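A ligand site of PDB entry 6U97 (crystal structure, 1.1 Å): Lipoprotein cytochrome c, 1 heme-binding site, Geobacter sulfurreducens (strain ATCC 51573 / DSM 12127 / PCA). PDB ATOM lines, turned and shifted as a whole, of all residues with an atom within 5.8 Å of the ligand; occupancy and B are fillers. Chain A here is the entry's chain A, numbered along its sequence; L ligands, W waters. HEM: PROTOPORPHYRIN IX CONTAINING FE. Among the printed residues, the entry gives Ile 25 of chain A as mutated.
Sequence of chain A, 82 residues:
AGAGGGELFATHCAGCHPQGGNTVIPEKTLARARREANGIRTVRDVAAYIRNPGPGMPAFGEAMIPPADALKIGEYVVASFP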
ATOM      1  N   PHE A   9     -20.430  32.606 -21.885  1.00  0.00           N
ATOM      2  CA  PHE A   9     -20.928  31.463 -21.130  1.00  0.00           C
ATOM      3  C   PHE A   9     -22.130  30.821 -21.806  1.00  0.00           C
ATOM      4  O   PHE A   9     -22.204  29.591 -21.907  1.00  0.00           O
ATOM      5  CB  PHE A   9     -21.271  31.892 -19.690  1.00  0.00           C
ATOM      6  CG  PHE A   9     -21.647  30.754 -18.827  1.00  0.00           C
ATOM      7  CD1 PHE A   9     -22.937  30.255 -18.785  1.00  0.00           C
ATOM      8  CD2 PHE A   9     -20.690  30.131 -18.008  1.00  0.00           C
ATOM      9  CE1 PHE A   9     -23.274  29.175 -17.953  1.00  0.00           C
ATOM     10  CE2 PHE A   9     -21.035  29.045 -17.198  1.00  0.00           C
ATOM     11  CZ  PHE A   9     -22.325  28.585 -17.177  1.00  0.00           C
ATOM     12  N   HIS A  12     -20.627  28.889 -24.891  1.00  0.00           N
ATOM     13  CA  HIS A  12     -19.668  27.816 -24.764  1.00  0.00           C
ATOM     14  C   HIS A  12     -19.920  26.890 -23.585  1.00  0.00           C
ATOM     15  O   HIS A  12     -19.367  25.789 -23.592  1.00  0.00           O
ATOM     16  CB  HIS A  12     -18.262  28.389 -24.585  1.00  0.00           C
ATOM     17  CG  HIS A  12     -17.774  29.144 -25.767  1.00  0.00           C
ATOM     18  ND1 HIS A  12     -17.474  28.532 -26.953  1.00  0.00           N
ATOM     19  CD2 HIS A  12     -17.544  30.462 -25.928  1.00  0.00           C
ATOM     20  CE1 HIS A  12     -17.094  29.458 -27.818  1.00  0.00           C
ATOM     21  NE2 HIS A  12     -17.098  30.626 -27.212  1.00  0.00           N
ATOM     22  N   CYS A  13     -20.693  27.295 -22.582  1.00  0.00           N
ATOM     23  CA  CYS A  13     -20.743  26.592 -21.307  1.00  0.00           C
ATOM     24  C   CYS A  13     -22.130  26.098 -20.913  1.00  0.00           C
ATOM     25  O   CYS A  13     -22.246  25.055 -20.265  1.00  0.00           O
ATOM     26  CB  CYS A  13     -20.153  27.437 -20.193  1.00  0.00           C
ATOM     27  SG  CYS A  13     -18.638  28.293 -20.579  1.00  0.00           S
ATOM     28  N   GLY A  15     -24.529  24.768 -22.402  1.00  0.00           N
ATOM     29  CA  GLY A  15     -24.997  23.486 -22.922  1.00  0.00           C
ATOM     30  C   GLY A  15     -24.760  22.319 -22.009  1.00  0.00           C
ATOM     31  O   GLY A  15     -25.420  21.292 -22.176  1.00  0.00           O
ATOM     32  N   CYS A  16     -23.794  22.432 -21.110  1.00  0.00           N
ATOM     33  CA  CYS A  16     -23.598  21.482 -20.035  1.00  0.00           C
ATOM     34  C   CYS A  16     -23.790  22.058 -18.655  1.00  0.00           C
ATOM     35  O   CYS A  16     -24.012  21.273 -17.741  1.00  0.00           O
ATOM     36  CB  CYS A  16     -22.190  20.892 -20.085  1.00  0.00           C
ATOM     37  SG  CYS A  16     -21.899  20.012 -21.652  1.00  0.00           S
ATOM     38  N   HIS A  17     -23.752  23.382 -18.489  1.00  0.00           N
ATOM     39  CA  HIS A  17     -23.940  23.993 -17.181  1.00  0.00           C
ATOM     40  C   HIS A  17     -25.074  25.004 -17.250  1.00  0.00           C
ATOM     41  O   HIS A  17     -24.882  26.163 -16.869  1.00  0.00           O
ATOM     42  CB  HIS A  17     -22.641  24.696 -16.773  1.00  0.00           C
ATOM     43  CG  HIS A  17     -21.457  23.800 -16.648  1.00  0.00           C
ATOM     44  ND1 HIS A  17     -21.308  22.862 -15.663  1.00  0.00           N
ATOM     45  CD2 HIS A  17     -20.321  23.783 -17.355  1.00  0.00           C
ATOM     46  CE1 HIS A  17     -20.142  22.279 -15.795  1.00  0.00           C
ATOM     47  NE2 HIS A  17     -19.503  22.819 -16.790  1.00  0.00           N
ATOM     48  N   ASN A  22     -25.003  20.985 -13.939  1.00  0.00           N
ATOM     49  CA  ASN A  22     -24.141  20.090 -14.716  1.00  0.00           C
ATOM     50  C   ASN A  22     -25.022  18.971 -15.236  1.00  0.00           C
ATOM     51  O   ASN A  22     -25.513  18.163 -14.461  1.00  0.00           O
ATOM     52  CB  ASN A  22     -22.982  19.533 -13.885  1.00  0.00           C
ATOM     53  CG  ASN A  22     -21.917  18.884 -14.745  1.00  0.00           C
ATOM     54  OD1 ASN A  22     -22.216  18.189 -15.692  1.00  0.00           O
ATOM     55  ND2 ASN A  22     -20.660  19.153 -14.450  1.00  0.00           N
ATOM     56  N   VAL A  24     -24.006  16.556 -17.211  1.00  0.00           N
ATOM     57  CA  VAL A  24     -23.193  15.381 -17.487  1.00  0.00           C
ATOM     58  C   VAL A  24     -22.897  14.623 -16.221  1.00  0.00           C
ATOM     59  O   VAL A  24     -23.092  13.418 -16.173  1.00  0.00           O
ATOM     60  CB  VAL A  24     -21.912  15.750 -18.266  1.00  0.00           C
ATOM     61  CG1 VAL A  24     -21.120  14.527 -18.574  1.00  0.00           C
ATOM     62  CG2 VAL A  24     -22.292  16.435 -19.580  1.00  0.00           C
ATOM     63  N   ILE A  25     -22.360  15.329 -15.218  1.00  0.00           N
ATOM     64  CA  ILE A  25     -22.055  14.772 -13.902  1.00  0.00           C
ATOM     65  C   ILE A  25     -22.763  15.684 -12.910  1.00  0.00           C
ATOM     66  O   ILE A  25     -22.237  16.746 -12.526  1.00  0.00           O
ATOM     67  CB  ILE A  25     -20.536  14.705 -13.673  1.00  0.00           C
ATOM     68  CG1 ILE A  25     -19.859  13.870 -14.785  1.00  0.00           C
ATOM     69  CG2 ILE A  25     -20.269  14.102 -12.299  1.00  0.00           C
ATOM     70  CD1 ILE A  25     -18.449  13.567 -14.560  1.00  0.00           C
ATOM     71  N   LYS A  28     -21.253  17.913 -10.009  1.00  0.00           N
ATOM     72  CA  LYS A  28     -20.179  18.863 -10.337  1.00  0.00           C
ATOM     73  C   LYS A  28     -20.728  20.176 -10.894  1.00  0.00           C
ATOM     74  O   LYS A  28     -20.412  20.581 -12.000  1.00  0.00           O
ATOM     75  CB  LYS A  28     -19.194  18.215 -11.299  1.00  0.00           C
ATOM     76  CG  LYS A  28     -18.256  17.202 -10.704  1.00  0.00           C
ATOM     77  CD  LYS A  28     -17.111  17.881  -9.928  1.00  0.00           C
ATOM     78  CE  LYS A  28     -15.967  17.033  -9.672  1.00  0.00           C
ATOM     79  NZ  LYS A  28     -15.002  17.744  -8.905  1.00  0.00           N
ATOM     80  N   THR A  29     -21.557  20.836 -10.095  1.00  0.00           N
ATOM     81  CA  THR A  29     -22.105  22.111 -10.515  1.00  0.00           C
ATOM     82  C   THR A  29     -21.099  23.240 -10.273  1.00  0.00           C
ATOM     83  O   THR A  29     -20.056  23.078  -9.657  1.00  0.00           O
ATOM     84  CB  THR A  29     -23.453  22.408  -9.869  1.00  0.00           C
ATOM     85  OG1 THR A  29     -23.202  22.796  -8.525  1.00  0.00           O
ATOM     86  CG2 THR A  29     -24.453  21.237  -9.907  1.00  0.00           C
ATOM     87  N   LEU A  30     -21.458  24.422 -10.760  1.00  0.00           N
ATOM     88  CA  LEU A  30     -20.622  25.601 -10.629  1.00  0.00           C
ATOM     89  C   LEU A  30     -20.856  26.354  -9.337  1.00  0.00           C
ATOM     90  O   LEU A  30     -20.247  27.397  -9.116  1.00  0.00           O
ATOM     91  CB  LEU A  30     -20.772  26.511 -11.835  1.00  0.00           C
ATOM     92  CG  LEU A  30     -20.634  25.825 -13.184  1.00  0.00           C
ATOM     93  CD1 LEU A  30     -20.580  26.878 -14.303  1.00  0.00           C
ATOM     94  CD2 LEU A  30     -19.431  24.976 -13.237  1.00  0.00           C
ATOM     95  N   ARG A  34     -19.150  24.204  -4.085  1.00  0.00           N
ATOM     96  CA  ARG A  34     -18.740  22.996  -4.793  1.00  0.00           C
ATOM     97  C   ARG A  34     -17.454  23.245  -5.574  1.00  0.00           C
ATOM     98  O   ARG A  34     -16.490  22.480  -5.458  1.00  0.00           O
ATOM     99  CB  ARG A  34     -19.859  22.490  -5.701  1.00  0.00           C
ATOM    100  CG  ARG A  34     -21.146  22.203  -4.957  1.00  0.00           C
ATOM    101  CD  ARG A  34     -22.087  21.379  -5.804  1.00  0.00           C
ATOM    102  NE  ARG A  34     -23.448  21.399  -5.305  1.00  0.00           N
ATOM    103  CZ  ARG A  34     -24.383  20.523  -5.612  1.00  0.00           C
ATOM    104  NH1 ARG A  34     -24.110  19.506  -6.403  1.00  0.00           N
ATOM    105  NH2 ARG A  34     -25.610  20.665  -5.130  1.00  0.00           N
ATOM    106  N   ARG A  35     -17.429  24.298  -6.385  1.00  0.00           N
ATOM    107  CA  ARG A  35     -16.243  24.578  -7.189  1.00  0.00           C
ATOM    108  C   ARG A  35     -15.037  24.933  -6.321  1.00  0.00           C
ATOM    109  O   ARG A  35     -13.923  24.535  -6.615  1.00  0.00           O
ATOM    110  CB  ARG A  35     -16.522  25.650  -8.248  1.00  0.00           C
ATOM    111  CG  ARG A  35     -16.740  27.021  -7.721  1.00  0.00           C
ATOM    112  CD  ARG A  35     -16.775  28.136  -8.808  1.00  0.00           C
ATOM    113  NE  ARG A  35     -16.776  29.484  -8.157  1.00  0.00           N
ATOM    114  CZ  ARG A  35     -17.850  30.226  -7.926  1.00  0.00           C
ATOM    115  NH1 ARG A  35     -17.716  31.383  -7.308  1.00  0.00           N
ATOM    116  NH2 ARG A  35     -19.065  29.857  -8.291  1.00  0.00           N
ATOM    117  N   ASN A  38     -12.881  22.194  -4.895  1.00  0.00           N
ATOM    118  CA  ASN A  38     -11.922  21.672  -5.867  1.00  0.00           C
ATOM    119  C   ASN A  38     -10.927  22.740  -6.322  1.00  0.00           C
ATOM    120  O   ASN A  38     -10.286  22.587  -7.353  1.00  0.00           O
ATOM    121  CB  ASN A  38     -12.648  21.031  -7.060  1.00  0.00           C
ATOM    122  CG  ASN A  38     -13.710  19.954  -6.623  1.00  0.00           C
ATOM    123  OD1 ASN A  38     -13.361  18.832  -6.249  1.00  0.00           O
ATOM    124  ND2 ASN A  38     -14.997  20.324  -6.668  1.00  0.00           N
ATOM    125  N   ILE A  40     -11.350  25.989  -7.304  1.00  0.00           N
ATOM    126  CA  ILE A  40     -11.721  26.903  -8.369  1.00  0.00           C
ATOM    127  C   ILE A  40     -12.425  28.070  -7.679  1.00  0.00           C
ATOM    128  O   ILE A  40     -13.649  28.103  -7.521  1.00  0.00           O
ATOM    129  CB  ILE A  40     -12.577  26.215  -9.425  1.00  0.00           C
ATOM    130  CG1 ILE A  40     -11.841  24.985  -9.932  1.00  0.00           C
ATOM    131  CG2 ILE A  40     -12.915  27.205 -10.511  1.00  0.00           C
ATOM    132  CD1 ILE A  40     -12.695  24.050 -10.687  1.00  0.00           C
ATOM    133  N   VAL A  46     -10.743  29.907 -12.825  1.00  0.00           N
ATOM    134  CA  VAL A  46     -11.696  29.444 -13.819  1.00  0.00           C
ATOM    135  C   VAL A  46     -11.038  29.469 -15.210  1.00  0.00           C
ATOM    136  O   VAL A  46     -11.168  28.529 -15.992  1.00  0.00           O
ATOM    137  CB  VAL A  46     -12.988  30.288 -13.796  1.00  0.00           C
ATOM    138  CG1 VAL A  46     -13.874  29.832 -14.925  1.00  0.00           C
ATOM    139  CG2 VAL A  46     -13.706  30.143 -12.470  1.00  0.00           C
ATOM    140  N   TYR A  49      -8.716  26.590 -15.499  1.00  0.00           N
ATOM    141  CA  TYR A  49      -9.421  25.316 -15.482  1.00  0.00           C
ATOM    142  C   TYR A  49      -9.944  24.959 -16.873  1.00  0.00           C
ATOM    143  O   TYR A  49      -9.846  23.793 -17.287  1.00  0.00           O
ATOM    144  CB  TYR A  49     -10.575  25.349 -14.467  1.00  0.00           C
ATOM    145  CG  TYR A  49     -11.314  24.065 -14.403  1.00  0.00           C
ATOM    146  CD1 TYR A  49     -10.764  22.973 -13.772  1.00  0.00           C
ATOM    147  CD2 TYR A  49     -12.538  23.909 -15.045  1.00  0.00           C
ATOM    148  CE1 TYR A  49     -11.425  21.766 -13.751  1.00  0.00           C
ATOM    149  CE2 TYR A  49     -13.215  22.716 -15.057  1.00  0.00           C
ATOM    150  CZ  TYR A  49     -12.645  21.620 -14.414  1.00  0.00           C
ATOM    151  OH  TYR A  49     -13.300  20.407 -14.456  1.00  0.00           O
ATOM    152  N   ILE A  50     -10.531  25.899 -17.603  1.00  0.00           N
ATOM    153  CA  ILE A  50     -11.105  25.548 -18.873  1.00  0.00           C
ATOM    154  C   ILE A  50     -10.080  25.126 -19.907  1.00  0.00           C
ATOM    155  O   ILE A  50     -10.448  24.423 -20.836  1.00  0.00           O
ATOM    156  CB  ILE A  50     -11.993  26.675 -19.447  1.00  0.00           C
ATOM    157  CG1 ILE A  50     -11.181  27.882 -19.915  1.00  0.00           C
ATOM    158  CG2 ILE A  50     -13.068  27.059 -18.474  1.00  0.00           C
ATOM    159  CD1 ILE A  50     -11.956  29.019 -20.550  1.00  0.00           C
ATOM    160  N   PRO A  53      -9.579  20.801 -18.230  1.00  0.00           N
ATOM    161  CA  PRO A  53     -10.611  20.471 -17.237  1.00  0.00           C
ATOM    162  C   PRO A  53     -10.694  18.980 -16.977  1.00  0.00           C
ATOM    163  O   PRO A  53      -9.976  18.180 -17.555  1.00  0.00           O
ATOM    164  CB  PRO A  53     -11.861  21.002 -17.905  1.00  0.00           C
ATOM    165  CG  PRO A  53     -11.616  20.746 -19.362  1.00  0.00           C
ATOM    166  CD  PRO A  53     -10.166  21.058 -19.563  1.00  0.00           C
ATOM    167  N   GLY A  54     -11.593  18.591 -16.082  1.00  0.00           N
ATOM    168  CA  GLY A  54     -11.771  17.218 -15.720  1.00  0.00           C
ATOM    169  C   GLY A  54     -12.477  16.393 -16.771  1.00  0.00           C
ATOM    170  O   GLY A  54     -12.951  16.897 -17.782  1.00  0.00           O
ATOM    171  N   PRO A  55     -12.506  15.090 -16.546  1.00  0.00           N
ATOM    172  CA  PRO A  55     -13.081  14.194 -17.570  1.00  0.00           C
ATOM    173  C   PRO A  55     -14.543  14.513 -17.857  1.00  0.00           C
ATOM    174  O   PRO A  55     -15.311  14.797 -16.951  1.00  0.00           O
ATOM    175  CB  PRO A  55     -12.912  12.807 -16.932  1.00  0.00           C
ATOM    176  CG  PRO A  55     -11.771  12.956 -15.984  1.00  0.00           C
ATOM    177  CD  PRO A  55     -11.916  14.346 -15.425  1.00  0.00           C
ATOM    178  N   GLY A  56     -14.899  14.448 -19.119  1.00  0.00           N
ATOM    179  CA  GLY A  56     -16.251  14.700 -19.602  1.00  0.00           C
ATOM    180  C   GLY A  56     -16.466  16.139 -20.045  1.00  0.00           C
ATOM    181  O   GLY A  56     -17.524  16.446 -20.563  1.00  0.00           O
ATOM    182  N   MET A  57     -15.525  17.024 -19.761  1.00  0.00           N
ATOM    183  CA  MET A  57     -15.550  18.409 -20.198  1.00  0.00           C
ATOM    184  C   MET A  57     -14.469  18.631 -21.245  1.00  0.00           C
ATOM    185  O   MET A  57     -13.318  18.259 -21.042  1.00  0.00           O
ATOM    186  CB  MET A  57     -15.269  19.318 -19.019  1.00  0.00           C
ATOM    187  CG  MET A  57     -15.287  20.789 -19.403  1.00  0.00           C
ATOM    188  SD  MET A  57     -15.395  21.881 -17.946  1.00  0.00           S
ATOM    189  CE  MET A  57     -14.592  23.303 -18.573  1.00  0.00           C
ATOM    190  N   PRO A  58     -14.796  19.221 -22.373  1.00  0.00           N
ATOM    191  CA  PRO A  58     -13.752  19.474 -23.366  1.00  0.00           C
ATOM    192  C   PRO A  58     -12.852  20.603 -22.911  1.00  0.00           C
ATOM    193  O   PRO A  58     -13.300  21.517 -22.229  1.00  0.00           O
ATOM    194  CB  PRO A  58     -14.533  19.882 -24.621  1.00  0.00           C
ATOM    195  CG  PRO A  58     -15.787  20.399 -24.110  1.00  0.00           C
ATOM    196  CD  PRO A  58     -16.120  19.658 -22.844  1.00  0.00           C
ATOM    197  N   PHE A  60     -10.889  24.012 -23.681  1.00  0.00           N
ATOM    198  CA  PHE A  60     -11.118  25.187 -24.478  1.00  0.00           C
ATOM    199  C   PHE A  60      -9.795  25.919 -24.609  1.00  0.00           C
ATOM    200  O   PHE A  60      -9.365  26.583 -23.677  1.00  0.00           O
ATOM    201  CB  PHE A  60     -12.162  26.090 -23.822  1.00  0.00           C
ATOM    202  CG  PHE A  60     -13.548  25.501 -23.805  1.00  0.00           C
ATOM    203  CD1 PHE A  60     -13.950  24.660 -22.769  1.00  0.00           C
ATOM    204  CD2 PHE A  60     -14.461  25.800 -24.805  1.00  0.00           C
ATOM    205  CE1 PHE A  60     -15.230  24.153 -22.746  1.00  0.00           C
ATOM    206  CE2 PHE A  60     -15.742  25.280 -24.787  1.00  0.00           C
ATOM    207  CZ  PHE A  60     -16.126  24.450 -23.778  1.00  0.00           C
ATOM    208  N   ILE A  65     -11.301  30.385 -27.233  1.00  0.00           N
ATOM    209  CA  ILE A  65     -11.591  31.314 -26.140  1.00  0.00           C
ATOM    210  C   ILE A  65     -10.281  32.046 -25.808  1.00  0.00           C
ATOM    211  O   ILE A  65      -9.477  31.525 -25.018  1.00  0.00           O
ATOM    212  CB  ILE A  65     -12.192  30.627 -24.902  1.00  0.00           C
ATOM    213  CG1 ILE A  65     -13.488  29.895 -25.275  1.00  0.00           C
ATOM    214  CG2 ILE A  65     -12.404  31.634 -23.792  1.00  0.00           C
ATOM    215  CD1 ILE A  65     -14.234  29.329 -24.134  1.00  0.00           C
ATOM    216  N   ILE A  73     -15.243  35.087 -18.843  1.00  0.00           N
ATOM    217  CA  ILE A  73     -15.990  33.929 -18.387  1.00  0.00           C
ATOM    218  C   ILE A  73     -15.785  33.705 -16.895  1.00  0.00           C
ATOM    219  O   ILE A  73     -16.737  33.477 -16.158  1.00  0.00           O
ATOM    220  CB  ILE A  73     -15.639  32.691 -19.231  1.00  0.00           C
ATOM    221  CG1 ILE A  73     -16.174  32.840 -20.654  1.00  0.00           C
ATOM    222  CG2 ILE A  73     -16.238  31.425 -18.628  1.00  0.00           C
ATOM    223  CD1 ILE A  73     -15.698  31.770 -21.597  1.00  0.00           C
ATOM    224  N   VAL A  77     -18.623  33.584 -13.972  1.00  0.00           N
ATOM    225  CA  VAL A  77     -18.860  32.421 -13.138  1.00  0.00           C
ATOM    226  C   VAL A  77     -18.818  32.802 -11.663  1.00  0.00           C
ATOM    227  O   VAL A  77     -19.678  32.418 -10.878  1.00  0.00           O
ATOM    228  CB  VAL A  77     -17.827  31.321 -13.465  1.00  0.00           C
ATOM    229  CG1 VAL A  77     -17.793  30.233 -12.390  1.00  0.00           C
ATOM    230  CG2 VAL A  77     -18.093  30.751 -14.790  1.00  0.00           C
HETATM  231  CHA HEM L   1     -16.904  20.785 -14.458  1.00  0.00           C
HETATM  232  CHB HEM L   1     -16.652  25.330 -16.019  1.00  0.00           C
HETATM  233  CHC HEM L   1     -18.062  23.918 -20.386  1.00  0.00           C
HETATM  234  CHD HEM L   1     -18.803  19.483 -18.633  1.00  0.00           C
HETATM  235  C1A HEM L   1     -16.758  22.148 -14.446  1.00  0.00           C
HETATM  236  C2A HEM L   1     -16.342  22.996 -13.342  1.00  0.00           C
HETATM  237  C3A HEM L   1     -16.199  24.227 -13.789  1.00  0.00           C
HETATM  238  C4A HEM L   1     -16.564  24.221 -15.200  1.00  0.00           C
HETATM  239  CMA HEM L   1     -15.798  25.449 -13.002  1.00  0.00           C
HETATM  240  CAA HEM L   1     -16.131  22.466 -11.924  1.00  0.00           C
HETATM  241  CBA HEM L   1     -14.942  21.579 -11.762  1.00  0.00           C
HETATM  242  CGA HEM L   1     -14.807  20.970 -10.375  1.00  0.00           C
HETATM  243  O1A HEM L   1     -15.545  21.346  -9.412  1.00  0.00           O
HETATM  244  O2A HEM L   1     -13.944  20.041 -10.251  1.00  0.00           O
HETATM  245  C1B HEM L   1     -16.985  25.324 -17.352  1.00  0.00           C
HETATM  246  C2B HEM L   1     -16.983  26.514 -18.182  1.00  0.00           C
HETATM  247  C3B HEM L   1     -17.328  26.102 -19.408  1.00  0.00           C
HETATM  248  C4B HEM L   1     -17.600  24.700 -19.365  1.00  0.00           C
HETATM  249  CMB HEM L   1     -16.583  27.903 -17.706  1.00  0.00           C
HETATM  250  CAB HEM L   1     -17.369  26.933 -20.720  1.00  0.00           C
HETATM  251  CBB HEM L   1     -16.158  27.534 -21.083  1.00  0.00           C
HETATM  252  C1C HEM L   1     -18.428  22.583 -20.319  1.00  0.00           C
HETATM  253  C2C HEM L   1     -19.063  21.776 -21.338  1.00  0.00           C
HETATM  254  C3C HEM L   1     -19.300  20.571 -20.825  1.00  0.00           C
HETATM  255  C4C HEM L   1     -18.803  20.571 -19.454  1.00  0.00           C
HETATM  256  CMC HEM L   1     -19.405  22.311 -22.715  1.00  0.00           C
HETATM  257  CAC HEM L   1     -20.050  19.407 -21.459  1.00  0.00           C
HETATM  258  CBC HEM L   1     -19.678  18.930 -22.697  1.00  0.00           C
HETATM  259  C1D HEM L   1     -18.287  19.415 -17.357  1.00  0.00           C
HETATM  260  C2D HEM L   1     -18.070  18.210 -16.601  1.00  0.00           C
HETATM  261  C3D HEM L   1     -17.511  18.574 -15.459  1.00  0.00           C
HETATM  262  C4D HEM L   1     -17.375  19.997 -15.465  1.00  0.00           C
HETATM  263  CMD HEM L   1     -18.409  16.784 -17.038  1.00  0.00           C
HETATM  264  CAD HEM L   1     -17.084  17.640 -14.323  1.00  0.00           C
HETATM  265  CBD HEM L   1     -15.578  17.347 -14.410  1.00  0.00           C
HETATM  266  CGD HEM L   1     -15.090  16.439 -13.339  1.00  0.00           C
HETATM  267  O1D HEM L   1     -13.928  16.567 -12.901  1.00  0.00           O
HETATM  268  O2D HEM L   1     -15.833  15.565 -12.869  1.00  0.00           O
HETATM  269  NA  HEM L   1     -16.919  22.938 -15.540  1.00  0.00           N
HETATM  270  NB  HEM L   1     -17.417  24.259 -18.075  1.00  0.00           N
HETATM  271  NC  HEM L   1     -18.309  21.815 -19.207  1.00  0.00           N
HETATM  272  ND  HEM L   1     -17.796  20.470 -16.665  1.00  0.00           N
HETATM  273 FE   HEM L   1     -17.605  22.375 -17.379  1.00  0.00          FE
HETATM  274  O   HOH W   1     -15.615  13.720 -10.861  1.00  0.00           O
HETATM  275  O   HOH W   2     -12.776  18.958 -12.347  1.00  0.00           O
HETATM  276  O   HOH W   3     -15.683  13.485 -14.634  1.00  0.00           O
HETATM  277  O   HOH W   4     -18.205  21.162  -8.753  1.00  0.00           O
HETATM  278  O   HOH W   5     -12.423  15.076 -11.284  1.00  0.00           O
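Merely in contact with the ligand: Asn 22 (3.4 Å), Leu 30 (3.4 Å), Tyr 49 (3.4 Å), Ile 40 (3.5 Å), His 12 (3.6 Å), Gly 54 (3.6 Å), Pro 55 (3.6 Å), Pro 58 (3.6 Å), Gly 56 (3.6 Å), Ile 73 (3.7 Å), Phe 60 (3.7 Å), Ile 50 (3.7 Å), Ile 25 (3.7 Å), Val 24 (3.8 Å) and Arg 35 (3.98 Å).
21 residues have an atom within 4 Å of the ligand: His 12, Cys 13, Cys 16, His 17, Asn 22, Val 24, Ile 25, Lys 28, Leu 30, Arg 35, Asn 38, Ile 40, Tyr 49, Ile 50, Gly 54, Pro 55, Gly 56, Met 57, Pro 58, Phe 60 and Ile 73.
The nearest printed residue that does not touch the ligand is Ile 65 (4.03 Å).
CAB of the ligand is covalently linked to SG of Cys 13.
A carbon (CAC) of the ligand is covalently linked to the side-chain sulfur (SG) of Cys 16, at 2.0 Å.
NE2 of His 17 binds FE of the ligand (2.0 Å).
SD of Met 57 binds FE of the ligand, at 2.3 Å.
The side-chain amino group of Lys 28 is in salt-bridge range of an oxygen (O2A) of the ligand, 2.9 Å away.
The side-chain amide nitrogen (ND2) of Asn 38 sits at hydrogen-bond distance from an oxygen (O1A) of the ligand, 3.0 Å away.
Water W2 bridges OH of Tyr 49 (2.6 Å) and O2A of the ligand (2.6 Å).
Water W3 bridges the backbone carbonyl oxygen of Pro 55 (2.7 Å) and an oxygen (O2D) of the ligand (2.7 Å).
Water W4 lies within hydrogen-bond range of an oxygen (O1A) of the ligand (2.7 Å) and the backbone carbonyl oxygen of Thr 29 (2.8 Å).
The side-chain amino group (NZ) of Lys 28 is in hydrogen-bond range of the side-chain amide oxygen (OD1) of Asn 38, 3.3 Å away.
The backbone carbonyl oxygen of Lys 28 sits at hydrogen-bond distance from the side-chain amide nitrogen of Asn 22 (2.8 Å).
The side-chain amide nitrogen (ND2) of Asn 38 is in hydrogen-bond range of the backbone carbonyl oxygen (O) of Arg 34, at 2.9 Å.
The backbone NH (N) of Ile 25 is in hydrogen-bond range of the side-chain amide oxygen (OD1) of Asn 22, 2.9 Å away.
N of Val 24 sits at hydrogen-bond distance from OD1 of Asn 22, at 2.9 Å.
The guanidinium group (NH2) of Arg 35 is in hydrogen-bond range of the backbone carbonyl oxygen (O) of Leu 30 (2.9 Å).
The backbone NH (N) of Ile 40 is in hydrogen-bond range of the backbone carbonyl oxygen (O) of Arg 35 (3.0 Å).
N of Phe 60 is in hydrogen-bond range of O of Ile 50 (2.9 Å).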
